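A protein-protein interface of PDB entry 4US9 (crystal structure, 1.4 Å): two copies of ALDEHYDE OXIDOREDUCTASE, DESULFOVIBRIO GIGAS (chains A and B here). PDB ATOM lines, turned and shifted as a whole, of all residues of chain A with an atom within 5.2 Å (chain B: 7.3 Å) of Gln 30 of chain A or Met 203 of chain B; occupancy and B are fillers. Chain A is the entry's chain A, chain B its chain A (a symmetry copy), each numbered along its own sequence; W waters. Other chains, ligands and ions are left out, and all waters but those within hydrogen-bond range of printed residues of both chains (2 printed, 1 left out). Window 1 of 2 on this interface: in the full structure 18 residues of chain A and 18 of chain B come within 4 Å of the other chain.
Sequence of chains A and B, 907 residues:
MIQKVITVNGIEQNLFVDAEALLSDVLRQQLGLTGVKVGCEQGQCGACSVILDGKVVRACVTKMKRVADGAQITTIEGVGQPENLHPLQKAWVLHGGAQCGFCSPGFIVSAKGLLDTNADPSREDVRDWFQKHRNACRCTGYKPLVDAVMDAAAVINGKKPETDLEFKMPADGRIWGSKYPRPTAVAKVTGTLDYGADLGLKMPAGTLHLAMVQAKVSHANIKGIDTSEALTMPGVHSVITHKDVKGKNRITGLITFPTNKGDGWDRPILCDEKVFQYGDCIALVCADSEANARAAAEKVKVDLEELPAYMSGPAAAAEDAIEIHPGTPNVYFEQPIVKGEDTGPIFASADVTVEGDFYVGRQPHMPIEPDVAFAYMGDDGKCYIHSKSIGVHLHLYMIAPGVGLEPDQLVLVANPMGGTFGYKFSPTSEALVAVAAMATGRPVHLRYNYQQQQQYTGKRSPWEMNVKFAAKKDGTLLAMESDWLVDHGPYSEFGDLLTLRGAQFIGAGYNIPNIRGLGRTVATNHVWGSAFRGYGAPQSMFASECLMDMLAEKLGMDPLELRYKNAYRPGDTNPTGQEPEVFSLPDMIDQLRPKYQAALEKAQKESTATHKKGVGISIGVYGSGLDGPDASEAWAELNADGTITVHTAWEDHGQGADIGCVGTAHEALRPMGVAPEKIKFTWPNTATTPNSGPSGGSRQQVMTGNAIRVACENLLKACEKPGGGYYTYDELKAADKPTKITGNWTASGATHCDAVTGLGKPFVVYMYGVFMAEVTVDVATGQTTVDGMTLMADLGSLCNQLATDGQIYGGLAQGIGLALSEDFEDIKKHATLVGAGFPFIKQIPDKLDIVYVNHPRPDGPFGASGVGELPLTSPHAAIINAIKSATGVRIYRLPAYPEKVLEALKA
The side-chain amide nitrogen of Gln 30 of chain A is in hydrogen-bond range of the backbone carbonyl oxygen of Lys 202 of chain B (2.9 Å).
The backbone carbonyl oxygen of Phe 16 of chain A lies within hydrogen-bond range of the side-chain amide nitrogen of Gln 30 of chain A (2.9 Å).
O of Pro 443 of chain B sits at hydrogen-bond distance from N of Leu 208 of chain B.
The backbone carbonyl oxygen of Pro 204 of chain B is in hydrogen-bond range of the side-chain hydroxyl of Thr 207 of chain B, 2.8 Å away.
Pro 204 of chain B touches Met 1 of chain A.
Met 1 of chain A touches Tyr 376 of chain B (SD to CG, 3.6 Å).
Met 1 of chain A touches Pro 443 of chain B (CE to CG, 3.5 Å).
Phe 16 of chain A touches Pro 204 of chain B (O to CD, 3.4 Å).
CZ of Phe 374 of chain B touches CZ of Phe 16 of chain A, 3.6 Å away.
Tyr 376 of chain B touches Phe 16 of chain A.
Met 203 of chain B touches Gln 30 of chain A (C to NE2, 3.7 Å).
Gln 30 of chain A touches Pro 204 of chain B.
Printed residues of chain B within 4 Å of Phe 16 of chain A: Pro 204, Phe 374 and Tyr 376.
Gln 29 of chain A touches none of the printed residues of chain B.
Printed residues of chain B within 4 Å of Gln 30 of chain A: Lys 202 (2.9 Å), Met 203 (3.7 Å) and Pro 204 (3.6 Å).
Printed residues of chain A within 4 Å of Lys 202 of chain B: Gln 30 (2.9 Å).
Met 203 of chain B touches just one residue of chain A: Gln 30.
Of the printed residues of chain A, Phe 374 of chain B touches Phe 16 (3.6 Å).
Printed residues of chain A within 4 Å of Tyr 376 of chain B: Met 1 and Phe 16.
Of the printed residues of chain A, Pro 443 of chain B touches Met 1.
The nearest residue of chain A that does not touch Met 203 of chain B is Met 1 of chain A (4.1 Å).
Hydrophobic or aromatic side chains of chain B that line the printed part of chain A: Pro 204, Phe 374, Tyr 376 and Pro 443.
Of the 11 printed residues of chain A, 3 touch a printed residue of chain B.
Hydrophobic or aromatic side chains of chain A that line the printed part of chain B: Met 1 and Phe 16.
Among the printed residues, no Asp or Glu carboxylate lies within 4 Å of a Lys or Arg side-chain nitrogen of the other chain.
1 position is printed for both chains.
Of the 9 pairs that touch across the chains among the printed residues, none has its exchanged pair printed and touching as well.
Water W2 lies within hydrogen-bond range of O of Lys 202 of chain B (2.8 Å) and N of Phe 16 of chain A (2.9 Å).
Water W1 bridges O of Gly 32 of chain B (2.8 Å) and O of Leu 31 of chain A (3.4 Å).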
ATOM      1  N   MET A   1      -5.928  29.080  10.028  1.00  0.00           N
ATOM      2  CA  MET A   1      -6.735  29.208   8.768  1.00  0.00           C
ATOM      3  C   MET A   1      -6.343  30.535   8.176  1.00  0.00           C
ATOM      4  O   MET A   1      -5.914  31.448   8.895  1.00  0.00           O
ATOM      5  CB  MET A   1      -8.236  29.174   9.125  1.00  0.00           C
ATOM      6  CG  MET A   1      -9.190  29.736   8.055  1.00  0.00           C
ATOM      7  SD  MET A   1     -10.909  29.338   8.411  1.00  0.00           S
ATOM      8  CE  MET A   1     -11.062  27.696   7.748  1.00  0.00           C
ATOM      9  N   PHE A  16     -11.626  30.312   2.325  1.00  0.00           N
ATOM     10  CA  PHE A  16     -11.139  30.097   3.682  1.00  0.00           C
ATOM     11  C   PHE A  16     -10.558  28.694   3.755  1.00  0.00           C
ATOM     12  O   PHE A  16     -11.287  27.705   3.572  1.00  0.00           O
ATOM     13  CB  PHE A  16     -12.272  30.312   4.664  1.00  0.00           C
ATOM     14  CG  PHE A  16     -12.703  31.755   4.664  1.00  0.00           C
ATOM     15  CD1 PHE A  16     -12.073  32.684   5.481  1.00  0.00           C
ATOM     16  CD2 PHE A  16     -13.659  32.201   3.773  1.00  0.00           C
ATOM     17  CE1 PHE A  16     -12.401  34.017   5.423  1.00  0.00           C
ATOM     18  CE2 PHE A  16     -13.978  33.537   3.694  1.00  0.00           C
ATOM     19  CZ  PHE A  16     -13.361  34.448   4.529  1.00  0.00           C
ATOM     20  N   VAL A  17      -9.244  28.636   3.968  1.00  0.00           N
ATOM     21  CA  VAL A  17      -8.506  27.396   3.829  1.00  0.00           C
ATOM     22  C   VAL A  17      -7.459  27.234   4.909  1.00  0.00           C
ATOM     23  O   VAL A  17      -6.988  28.197   5.508  1.00  0.00           O
ATOM     24  CB  VAL A  17      -7.834  27.258   2.443  1.00  0.00           C
ATOM     25  CG1 VAL A  17      -8.882  27.168   1.339  1.00  0.00           C
ATOM     26  CG2 VAL A  17      -6.850  28.394   2.204  1.00  0.00           C
ATOM     27  N   ASP A  25      -8.209  18.909  -2.843  1.00  0.00           N
ATOM     28  CA  ASP A  25      -9.292  18.799  -1.873  1.00  0.00           C
ATOM     29  C   ASP A  25     -10.094  20.090  -1.772  1.00  0.00           C
ATOM     30  O   ASP A  25     -11.324  20.063  -1.673  1.00  0.00           O
ATOM     31  CB  ASP A  25      -8.729  18.457  -0.490  1.00  0.00           C
ATOM     32  CG  ASP A  25      -8.191  17.042  -0.399  1.00  0.00           C
ATOM     33  OD1 ASP A  25      -8.692  16.147  -1.118  1.00  0.00           O
ATOM     34  OD2 ASP A  25      -7.278  16.824   0.424  1.00  0.00           O
ATOM     35  N   VAL A  26      -9.416  21.234  -1.768  1.00  0.00           N
ATOM     36  CA  VAL A  26     -10.137  22.512  -1.721  1.00  0.00           C
ATOM     37  C   VAL A  26     -11.069  22.637  -2.931  1.00  0.00           C
ATOM     38  O   VAL A  26     -12.249  22.966  -2.784  1.00  0.00           O
ATOM     39  CB  VAL A  26      -9.156  23.695  -1.639  1.00  0.00           C
ATOM     40  CG1 VAL A  26      -9.876  25.030  -1.759  1.00  0.00           C
ATOM     41  CG2 VAL A  26      -8.335  23.605  -0.344  1.00  0.00           C
ATOM     42  N   LEU A  27     -10.542  22.375  -4.125  1.00  0.00           N
ATOM     43  CA  LEU A  27     -11.331  22.511  -5.343  1.00  0.00           C
ATOM     44  C   LEU A  27     -12.502  21.531  -5.355  1.00  0.00           C
ATOM     45  O   LEU A  27     -13.651  21.922  -5.621  1.00  0.00           O
ATOM     46  CB  LEU A  27     -10.460  22.359  -6.592  1.00  0.00           C
ATOM     47  CG  LEU A  27      -9.392  23.453  -6.777  1.00  0.00           C
ATOM     48  CD1 LEU A  27      -8.517  23.116  -7.963  1.00  0.00           C
ATOM     49  CD2 LEU A  27     -10.014  24.813  -6.971  1.00  0.00           C
ATOM     50  N   ARG A  28     -12.221  20.252  -5.066  1.00  0.00           N
ATOM     51  CA  ARG A  28     -13.289  19.237  -5.128  1.00  0.00           C
ATOM     52  C   ARG A  28     -14.303  19.352  -4.000  1.00  0.00           C
ATOM     53  O   ARG A  28     -15.521  19.308  -4.240  1.00  0.00           O
ATOM     54  CB  ARG A  28     -12.700  17.822  -5.103  1.00  0.00           C
ATOM     55  CG  ARG A  28     -11.938  17.441  -6.361  1.00  0.00           C
ATOM     56  CD  ARG A  28     -11.244  16.073  -6.238  1.00  0.00           C
ATOM     57  NE  ARG A  28     -12.164  14.977  -5.928  1.00  0.00           N
ATOM     58  CZ  ARG A  28     -13.011  14.424  -6.797  1.00  0.00           C
ATOM     59  NH1 ARG A  28     -13.053  14.823  -8.069  1.00  0.00           N
ATOM     60  NH2 ARG A  28     -13.825  13.461  -6.392  1.00  0.00           N
ATOM     61  N   GLN A  29     -13.809  19.483  -2.765  1.00  0.00           N
ATOM     62  CA  GLN A  29     -14.680  19.390  -1.595  1.00  0.00           C
ATOM     63  C   GLN A  29     -15.263  20.740  -1.181  1.00  0.00           C
ATOM     64  O   GLN A  29     -16.449  20.866  -0.942  1.00  0.00           O
ATOM     65  CB  GLN A  29     -13.933  18.742  -0.441  1.00  0.00           C
ATOM     66  CG  GLN A  29     -13.325  17.398  -0.785  1.00  0.00           C
ATOM     67  CD  GLN A  29     -12.799  16.638   0.405  1.00  0.00           C
ATOM     68  OE1 GLN A  29     -13.443  16.559   1.445  1.00  0.00           O
ATOM     69  NE2 GLN A  29     -11.614  16.064   0.247  1.00  0.00           N
ATOM     70  N   GLN A  30     -14.434  21.766  -1.095  1.00  0.00           N
ATOM     71  CA  GLN A  30     -14.936  23.061  -0.682  1.00  0.00           C
ATOM     72  C   GLN A  30     -15.701  23.750  -1.786  1.00  0.00           C
ATOM     73  O   GLN A  30     -16.733  24.378  -1.526  1.00  0.00           O
ATOM     74  CB  GLN A  30     -13.821  23.956  -0.116  1.00  0.00           C
ATOM     75  CG  GLN A  30     -13.215  23.393   1.169  1.00  0.00           C
ATOM     76  CD  GLN A  30     -12.105  24.222   1.765  1.00  0.00           C
ATOM     77  OE1 GLN A  30     -10.986  23.735   1.928  1.00  0.00           O
ATOM     78  NE2 GLN A  30     -12.376  25.462   2.083  1.00  0.00           N
ATOM     79  N   LEU A  31     -15.205  23.648  -3.036  1.00  0.00           N
ATOM     80  CA  LEU A  31     -15.847  24.373  -4.153  1.00  0.00           C
ATOM     81  C   LEU A  31     -16.690  23.494  -5.063  1.00  0.00           C
ATOM     82  O   LEU A  31     -17.310  24.007  -5.968  1.00  0.00           O
ATOM     83  CB  LEU A  31     -14.806  25.129  -4.974  1.00  0.00           C
ATOM     84  CG  LEU A  31     -13.967  26.134  -4.161  1.00  0.00           C
ATOM     85  CD1 LEU A  31     -13.008  26.910  -5.059  1.00  0.00           C
ATOM     86  CD2 LEU A  31     -14.857  27.084  -3.348  1.00  0.00           C
ATOM     87  N   GLY A  32     -16.712  22.191  -4.848  1.00  0.00           N
ATOM     88  CA  GLY A  32     -17.565  21.323  -5.645  1.00  0.00           C
ATOM     89  C   GLY A  32     -17.083  21.038  -7.063  1.00  0.00           C
ATOM     90  O   GLY A  32     -17.873  20.577  -7.886  1.00  0.00           O
ATOM     91  N   GLY B  32     -23.572  21.989  -4.291  1.00  0.00           N
ATOM     92  CA  GLY B  32     -22.793  23.217  -4.272  1.00  0.00           C
ATOM     93  C   GLY B  32     -23.467  24.442  -4.882  1.00  0.00           C
ATOM     94  O   GLY B  32     -22.784  25.421  -5.179  1.00  0.00           O
ATOM     95  N   GLY B 196     -22.586  34.992   4.264  1.00  0.00           N
ATOM     96  CA  GLY B 196     -21.996  34.211   5.340  1.00  0.00           C
ATOM     97  C   GLY B 196     -22.393  32.745   5.415  1.00  0.00           C
ATOM     98  O   GLY B 196     -21.555  31.906   5.738  1.00  0.00           O
ATOM     99  N   ASP B 198     -23.285  30.884   2.861  1.00  0.00           N
ATOM    100  CA  ASP B 198     -22.630  30.306   1.680  1.00  0.00           C
ATOM    101  C   ASP B 198     -21.169  29.962   2.008  1.00  0.00           C
ATOM    102  O   ASP B 198     -20.651  28.882   1.704  1.00  0.00           O
ATOM    103  CB  ASP B 198     -22.681  31.285   0.495  1.00  0.00           C
ATOM    104  CG  ASP B 198     -24.092  31.779   0.147  1.00  0.00           C
ATOM    105  OD1 ASP B 198     -25.032  30.953   0.320  1.00  0.00           O
ATOM    106  OD2 ASP B 198     -24.249  32.925  -0.281  1.00  0.00           O
ATOM    107  N   LEU B 199     -20.486  30.925   2.639  1.00  0.00           N
ATOM    108  CA  LEU B 199     -19.087  30.747   3.050  1.00  0.00           C
ATOM    109  C   LEU B 199     -18.969  29.571   4.017  1.00  0.00           C
ATOM    110  O   LEU B 199     -18.037  28.762   3.927  1.00  0.00           O
ATOM    111  CB  LEU B 199     -18.553  32.039   3.649  1.00  0.00           C
ATOM    112  CG  LEU B 199     -18.420  33.213   2.655  1.00  0.00           C
ATOM    113  CD1 LEU B 199     -18.125  34.497   3.386  1.00  0.00           C
ATOM    114  CD2 LEU B 199     -17.358  32.945   1.589  1.00  0.00           C
ATOM    115  N   GLY B 200     -19.935  29.425   4.925  1.00  0.00           N
ATOM    116  CA  GLY B 200     -19.907  28.283   5.830  1.00  0.00           C
ATOM    117  C   GLY B 200     -19.916  26.943   5.120  1.00  0.00           C
ATOM    118  O   GLY B 200     -19.192  26.017   5.489  1.00  0.00           O
ATOM    119  N   LEU B 201     -20.679  26.833   4.033  1.00  0.00           N
ATOM    120  CA  LEU B 201     -20.705  25.569   3.270  1.00  0.00           C
ATOM    121  C   LEU B 201     -19.397  25.306   2.522  1.00  0.00           C
ATOM    122  O   LEU B 201     -19.104  24.163   2.167  1.00  0.00           O
ATOM    123  CB  LEU B 201     -21.858  25.604   2.267  1.00  0.00           C
ATOM    124  CG  LEU B 201     -23.257  25.504   2.881  1.00  0.00           C
ATOM    125  CD1 LEU B 201     -24.324  25.427   1.802  1.00  0.00           C
ATOM    126  CD2 LEU B 201     -23.400  24.356   3.871  1.00  0.00           C
ATOM    127  N   LYS B 202     -18.606  26.359   2.328  1.00  0.00           N
ATOM    128  CA  LYS B 202     -17.365  26.292   1.547  1.00  0.00           C
ATOM    129  C   LYS B 202     -16.125  26.348   2.450  1.00  0.00           C
ATOM    130  O   LYS B 202     -15.011  26.568   1.963  1.00  0.00           O
ATOM    131  CB  LYS B 202     -17.333  27.407   0.500  1.00  0.00           C
ATOM    132  CG  LYS B 202     -18.485  27.278  -0.470  1.00  0.00           C
ATOM    133  CD  LYS B 202     -18.504  28.353  -1.532  1.00  0.00           C
ATOM    134  CE  LYS B 202     -19.804  28.258  -2.304  1.00  0.00           C
ATOM    135  NZ  LYS B 202     -19.880  29.263  -3.386  1.00  0.00           N
ATOM    136  N   MET B 203     -16.323  26.207   3.759  1.00  0.00           N
ATOM    137  CA  MET B 203     -15.230  26.150   4.706  1.00  0.00           C
ATOM    138  C   MET B 203     -14.751  24.688   4.800  1.00  0.00           C
ATOM    139  O   MET B 203     -15.482  23.732   4.477  1.00  0.00           O
ATOM    140  CB  MET B 203     -15.666  26.722   6.079  1.00  0.00           C
ATOM    141  CG  MET B 203     -15.664  28.240   6.125  1.00  0.00           C
ATOM    142  SD  MET B 203     -16.396  28.962   7.604  1.00  0.00           S
ATOM    143  CE  MET B 203     -15.011  28.887   8.731  1.00  0.00           C
ATOM    144  N   PRO B 204     -13.560  24.496   5.308  1.00  0.00           N
ATOM    145  CA  PRO B 204     -13.016  23.139   5.317  1.00  0.00           C
ATOM    146  C   PRO B 204     -13.611  22.228   6.349  1.00  0.00           C
ATOM    147  O   PRO B 204     -14.178  22.686   7.330  1.00  0.00           O
ATOM    148  CB  PRO B 204     -11.546  23.342   5.598  1.00  0.00           C
ATOM    149  CG  PRO B 204     -11.389  24.645   6.202  1.00  0.00           C
ATOM    150  CD  PRO B 204     -12.617  25.481   5.826  1.00  0.00           C
ATOM    151  N   ALA B 205     -13.394  20.929   6.157  1.00  0.00           N
ATOM    152  CA  ALA B 205     -13.920  19.898   7.048  1.00  0.00           C
ATOM    153  C   ALA B 205     -13.609  20.081   8.539  1.00  0.00           C
ATOM    154  O   ALA B 205     -14.418  19.683   9.364  1.00  0.00           O
ATOM    155  CB  ALA B 205     -13.479  18.512   6.587  1.00  0.00           C
ATOM    156  N   GLY B 206     -12.478  20.699   8.893  1.00  0.00           N
ATOM    157  CA  GLY B 206     -12.171  20.983  10.326  1.00  0.00           C
ATOM    158  C   GLY B 206     -13.111  21.946  11.060  1.00  0.00           C
ATOM    159  O   GLY B 206     -13.093  22.067  12.290  1.00  0.00           O
ATOM    160  N   THR B 207     -13.915  22.662  10.296  1.00  0.00           N
ATOM    161  CA  THR B 207     -14.733  23.752  10.813  1.00  0.00           C
ATOM    162  C   THR B 207     -15.802  23.177  11.750  1.00  0.00           C
ATOM    163  O   THR B 207     -16.483  22.196  11.430  1.00  0.00           O
ATOM    164  CB  THR B 207     -15.378  24.536   9.665  1.00  0.00           C
ATOM    165  OG1 THR B 207     -14.352  25.073   8.824  1.00  0.00           O
ATOM    166  CG2 THR B 207     -16.252  25.646  10.179  1.00  0.00           C
ATOM    167  N   LEU B 208     -15.929  23.795  12.918  1.00  0.00           N
ATOM    168  CA  LEU B 208     -16.977  23.446  13.860  1.00  0.00           C
ATOM    169  C   LEU B 208     -18.190  24.362  13.618  1.00  0.00           C
ATOM    170  O   LEU B 208     -18.043  25.551  13.345  1.00  0.00           O
ATOM    171  CB  LEU B 208     -16.477  23.565  15.304  1.00  0.00           C
ATOM    172  CG  LEU B 208     -15.382  22.560  15.658  1.00  0.00           C
ATOM    173  CD1 LEU B 208     -14.782  22.895  17.023  1.00  0.00           C
ATOM    174  CD2 LEU B 208     -15.891  21.133  15.637  1.00  0.00           C
ATOM    175  N   HIS B 209     -19.373  23.773  13.667  1.00  0.00           N
ATOM    176  CA  HIS B 209     -20.623  24.491  13.530  1.00  0.00           C
ATOM    177  C   HIS B 209     -21.246  24.659  14.882  1.00  0.00           C
ATOM    178  O   HIS B 209     -21.274  23.724  15.683  1.00  0.00           O
ATOM    179  CB  HIS B 209     -21.513  23.731  12.550  1.00  0.00           C
ATOM    180  CG  HIS B 209     -20.972  23.761  11.163  1.00  0.00           C
ATOM    181  ND1 HIS B 209     -20.068  22.861  10.645  1.00  0.00           N
ATOM    182  CD2 HIS B 209     -21.145  24.701  10.216  1.00  0.00           C
ATOM    183  CE1 HIS B 209     -19.745  23.234   9.421  1.00  0.00           C
ATOM    184  NE2 HIS B 209     -20.391  24.344   9.139  1.00  0.00           N
ATOM    185  N   ALA B 373     -22.241  34.460  11.166  1.00  0.00           N
ATOM    186  CA  ALA B 373     -20.857  34.918  11.345  1.00  0.00           C
ATOM    187  C   ALA B 373     -19.969  33.691  11.504  1.00  0.00           C
ATOM    188  O   ALA B 373     -20.435  32.584  11.839  1.00  0.00           O
ATOM    189  CB  ALA B 373     -20.736  35.804  12.577  1.00  0.00           C
ATOM    190  N   PHE B 374     -18.669  33.907  11.328  1.00  0.00           N
ATOM    191  CA  PHE B 374     -17.683  32.859  11.586  1.00  0.00           C
ATOM    192  C   PHE B 374     -16.406  33.483  12.109  1.00  0.00           C
ATOM    193  O   PHE B 374     -16.177  34.687  11.970  1.00  0.00           O
ATOM    194  CB  PHE B 374     -17.490  31.919  10.376  1.00  0.00           C
ATOM    195  CG  PHE B 374     -17.031  32.575   9.101  1.00  0.00           C
ATOM    196  CD1 PHE B 374     -17.937  33.048   8.179  1.00  0.00           C
ATOM    197  CD2 PHE B 374     -15.672  32.678   8.796  1.00  0.00           C
ATOM    198  CE1 PHE B 374     -17.503  33.598   6.986  1.00  0.00           C
ATOM    199  CE2 PHE B 374     -15.237  33.218   7.615  1.00  0.00           C
ATOM    200  CZ  PHE B 374     -16.157  33.668   6.705  1.00  0.00           C
ATOM    201  N   ALA B 375     -15.552  32.634  12.700  1.00  0.00           N
ATOM    202  CA  ALA B 375     -14.275  33.111  13.232  1.00  0.00           C
ATOM    203  C   ALA B 375     -13.253  32.002  13.165  1.00  0.00           C
ATOM    204  O   ALA B 375     -13.607  30.821  13.089  1.00  0.00           O
ATOM    205  CB  ALA B 375     -14.419  33.606  14.655  1.00  0.00           C
ATOM    206  N   TYR B 376     -11.987  32.382  13.236  1.00  0.00           N
ATOM    207  CA  TYR B 376     -10.914  31.411  13.229  1.00  0.00           C
ATOM    208  C   TYR B 376      -9.677  32.068  13.801  1.00  0.00           C
ATOM    209  O   TYR B 376      -9.552  33.282  13.838  1.00  0.00           O
ATOM    210  CB  TYR B 376     -10.646  30.878  11.792  1.00  0.00           C
ATOM    211  CG  TYR B 376     -10.404  31.957  10.760  1.00  0.00           C
ATOM    212  CD1 TYR B 376      -9.129  32.435  10.512  1.00  0.00           C
ATOM    213  CD2 TYR B 376     -11.463  32.518  10.042  1.00  0.00           C
ATOM    214  CE1 TYR B 376      -8.917  33.457   9.590  1.00  0.00           C
ATOM    215  CE2 TYR B 376     -11.253  33.528   9.128  1.00  0.00           C
ATOM    216  CZ  TYR B 376      -9.986  34.029   8.932  1.00  0.00           C
ATOM    217  OH  TYR B 376      -9.771  35.044   8.044  1.00  0.00           O
ATOM    218  N   ARG B 442     -10.115  26.172  16.623  1.00  0.00           N
ATOM    219  CA  ARG B 442     -10.611  25.680  15.344  1.00  0.00           C
ATOM    220  C   ARG B 442     -11.495  26.768  14.690  1.00  0.00           C
ATOM    221  O   ARG B 442     -12.036  27.638  15.377  1.00  0.00           O
ATOM    222  CB  ARG B 442     -11.468  24.429  15.543  1.00  0.00           C
ATOM    223  CG  ARG B 442     -10.793  23.257  16.243  1.00  0.00           C
ATOM    224  CD  ARG B 442     -10.395  22.174  15.307  1.00  0.00           C
ATOM    225  NE  ARG B 442     -11.475  21.467  14.625  1.00  0.00           N
ATOM    226  CZ  ARG B 442     -11.978  20.268  14.940  1.00  0.00           C
ATOM    227  NH1 ARG B 442     -11.610  19.607  16.034  1.00  0.00           N
ATOM    228  NH2 ARG B 442     -12.925  19.753  14.155  1.00  0.00           N
ATOM    229  N   PRO B 443     -11.651  26.721  13.356  1.00  0.00           N
ATOM    230  CA  PRO B 443     -12.642  27.588  12.744  1.00  0.00           C
ATOM    231  C   PRO B 443     -14.033  27.223  13.239  1.00  0.00           C
ATOM    232  O   PRO B 443     -14.336  26.030  13.428  1.00  0.00           O
ATOM    233  CB  PRO B 443     -12.484  27.302  11.232  1.00  0.00           C
ATOM    234  CG  PRO B 443     -11.123  26.683  11.086  1.00  0.00           C
ATOM    235  CD  PRO B 443     -10.990  25.879  12.342  1.00  0.00           C
ATOM    236  N   VAL B 444     -14.859  28.251  13.438  1.00  0.00           N
ATOM    237  CA  VAL B 444     -16.223  28.060  13.926  1.00  0.00           C
ATOM    238  C   VAL B 444     -17.172  28.896  13.078  1.00  0.00           C
ATOM    239  O   VAL B 444     -16.828  29.994  12.630  1.00  0.00           O
ATOM    240  CB  VAL B 444     -16.379  28.413  15.426  1.00  0.00           C
ATOM    241  CG1 VAL B 444     -15.415  27.576  16.262  1.00  0.00           C
ATOM    242  CG2 VAL B 444     -16.159  29.907  15.671  1.00  0.00           C
ATOM    243  N   HIS B 445     -18.381  28.372  12.893  1.00  0.00           N
ATOM    244  CA  HIS B 445     -19.411  29.053  12.093  1.00  0.00           C
ATOM    245  C   HIS B 445     -20.752  28.965  12.801  1.00  0.00           C
ATOM    246  O   HIS B 445     -21.144  27.881  13.268  1.00  0.00           O
ATOM    247  CB  HIS B 445     -19.484  28.403  10.688  1.00  0.00           C
ATOM    248  CG  HIS B 445     -20.367  29.116   9.724  1.00  0.00           C
ATOM    249  ND1 HIS B 445     -21.741  28.950   9.710  1.00  0.00           N
ATOM    250  CD2 HIS B 445     -20.079  30.009   8.748  1.00  0.00           C
ATOM    251  CE1 HIS B 445     -22.251  29.705   8.759  1.00  0.00           C
ATOM    252  NE2 HIS B 445     -21.271  30.360   8.164  1.00  0.00           N
HETATM  253  O   HOH W   1     -20.025  25.616  -4.635  1.00  0.00           O
HETATM  254  O   HOH W   2     -14.016  29.066   1.282  1.00  0.00           O
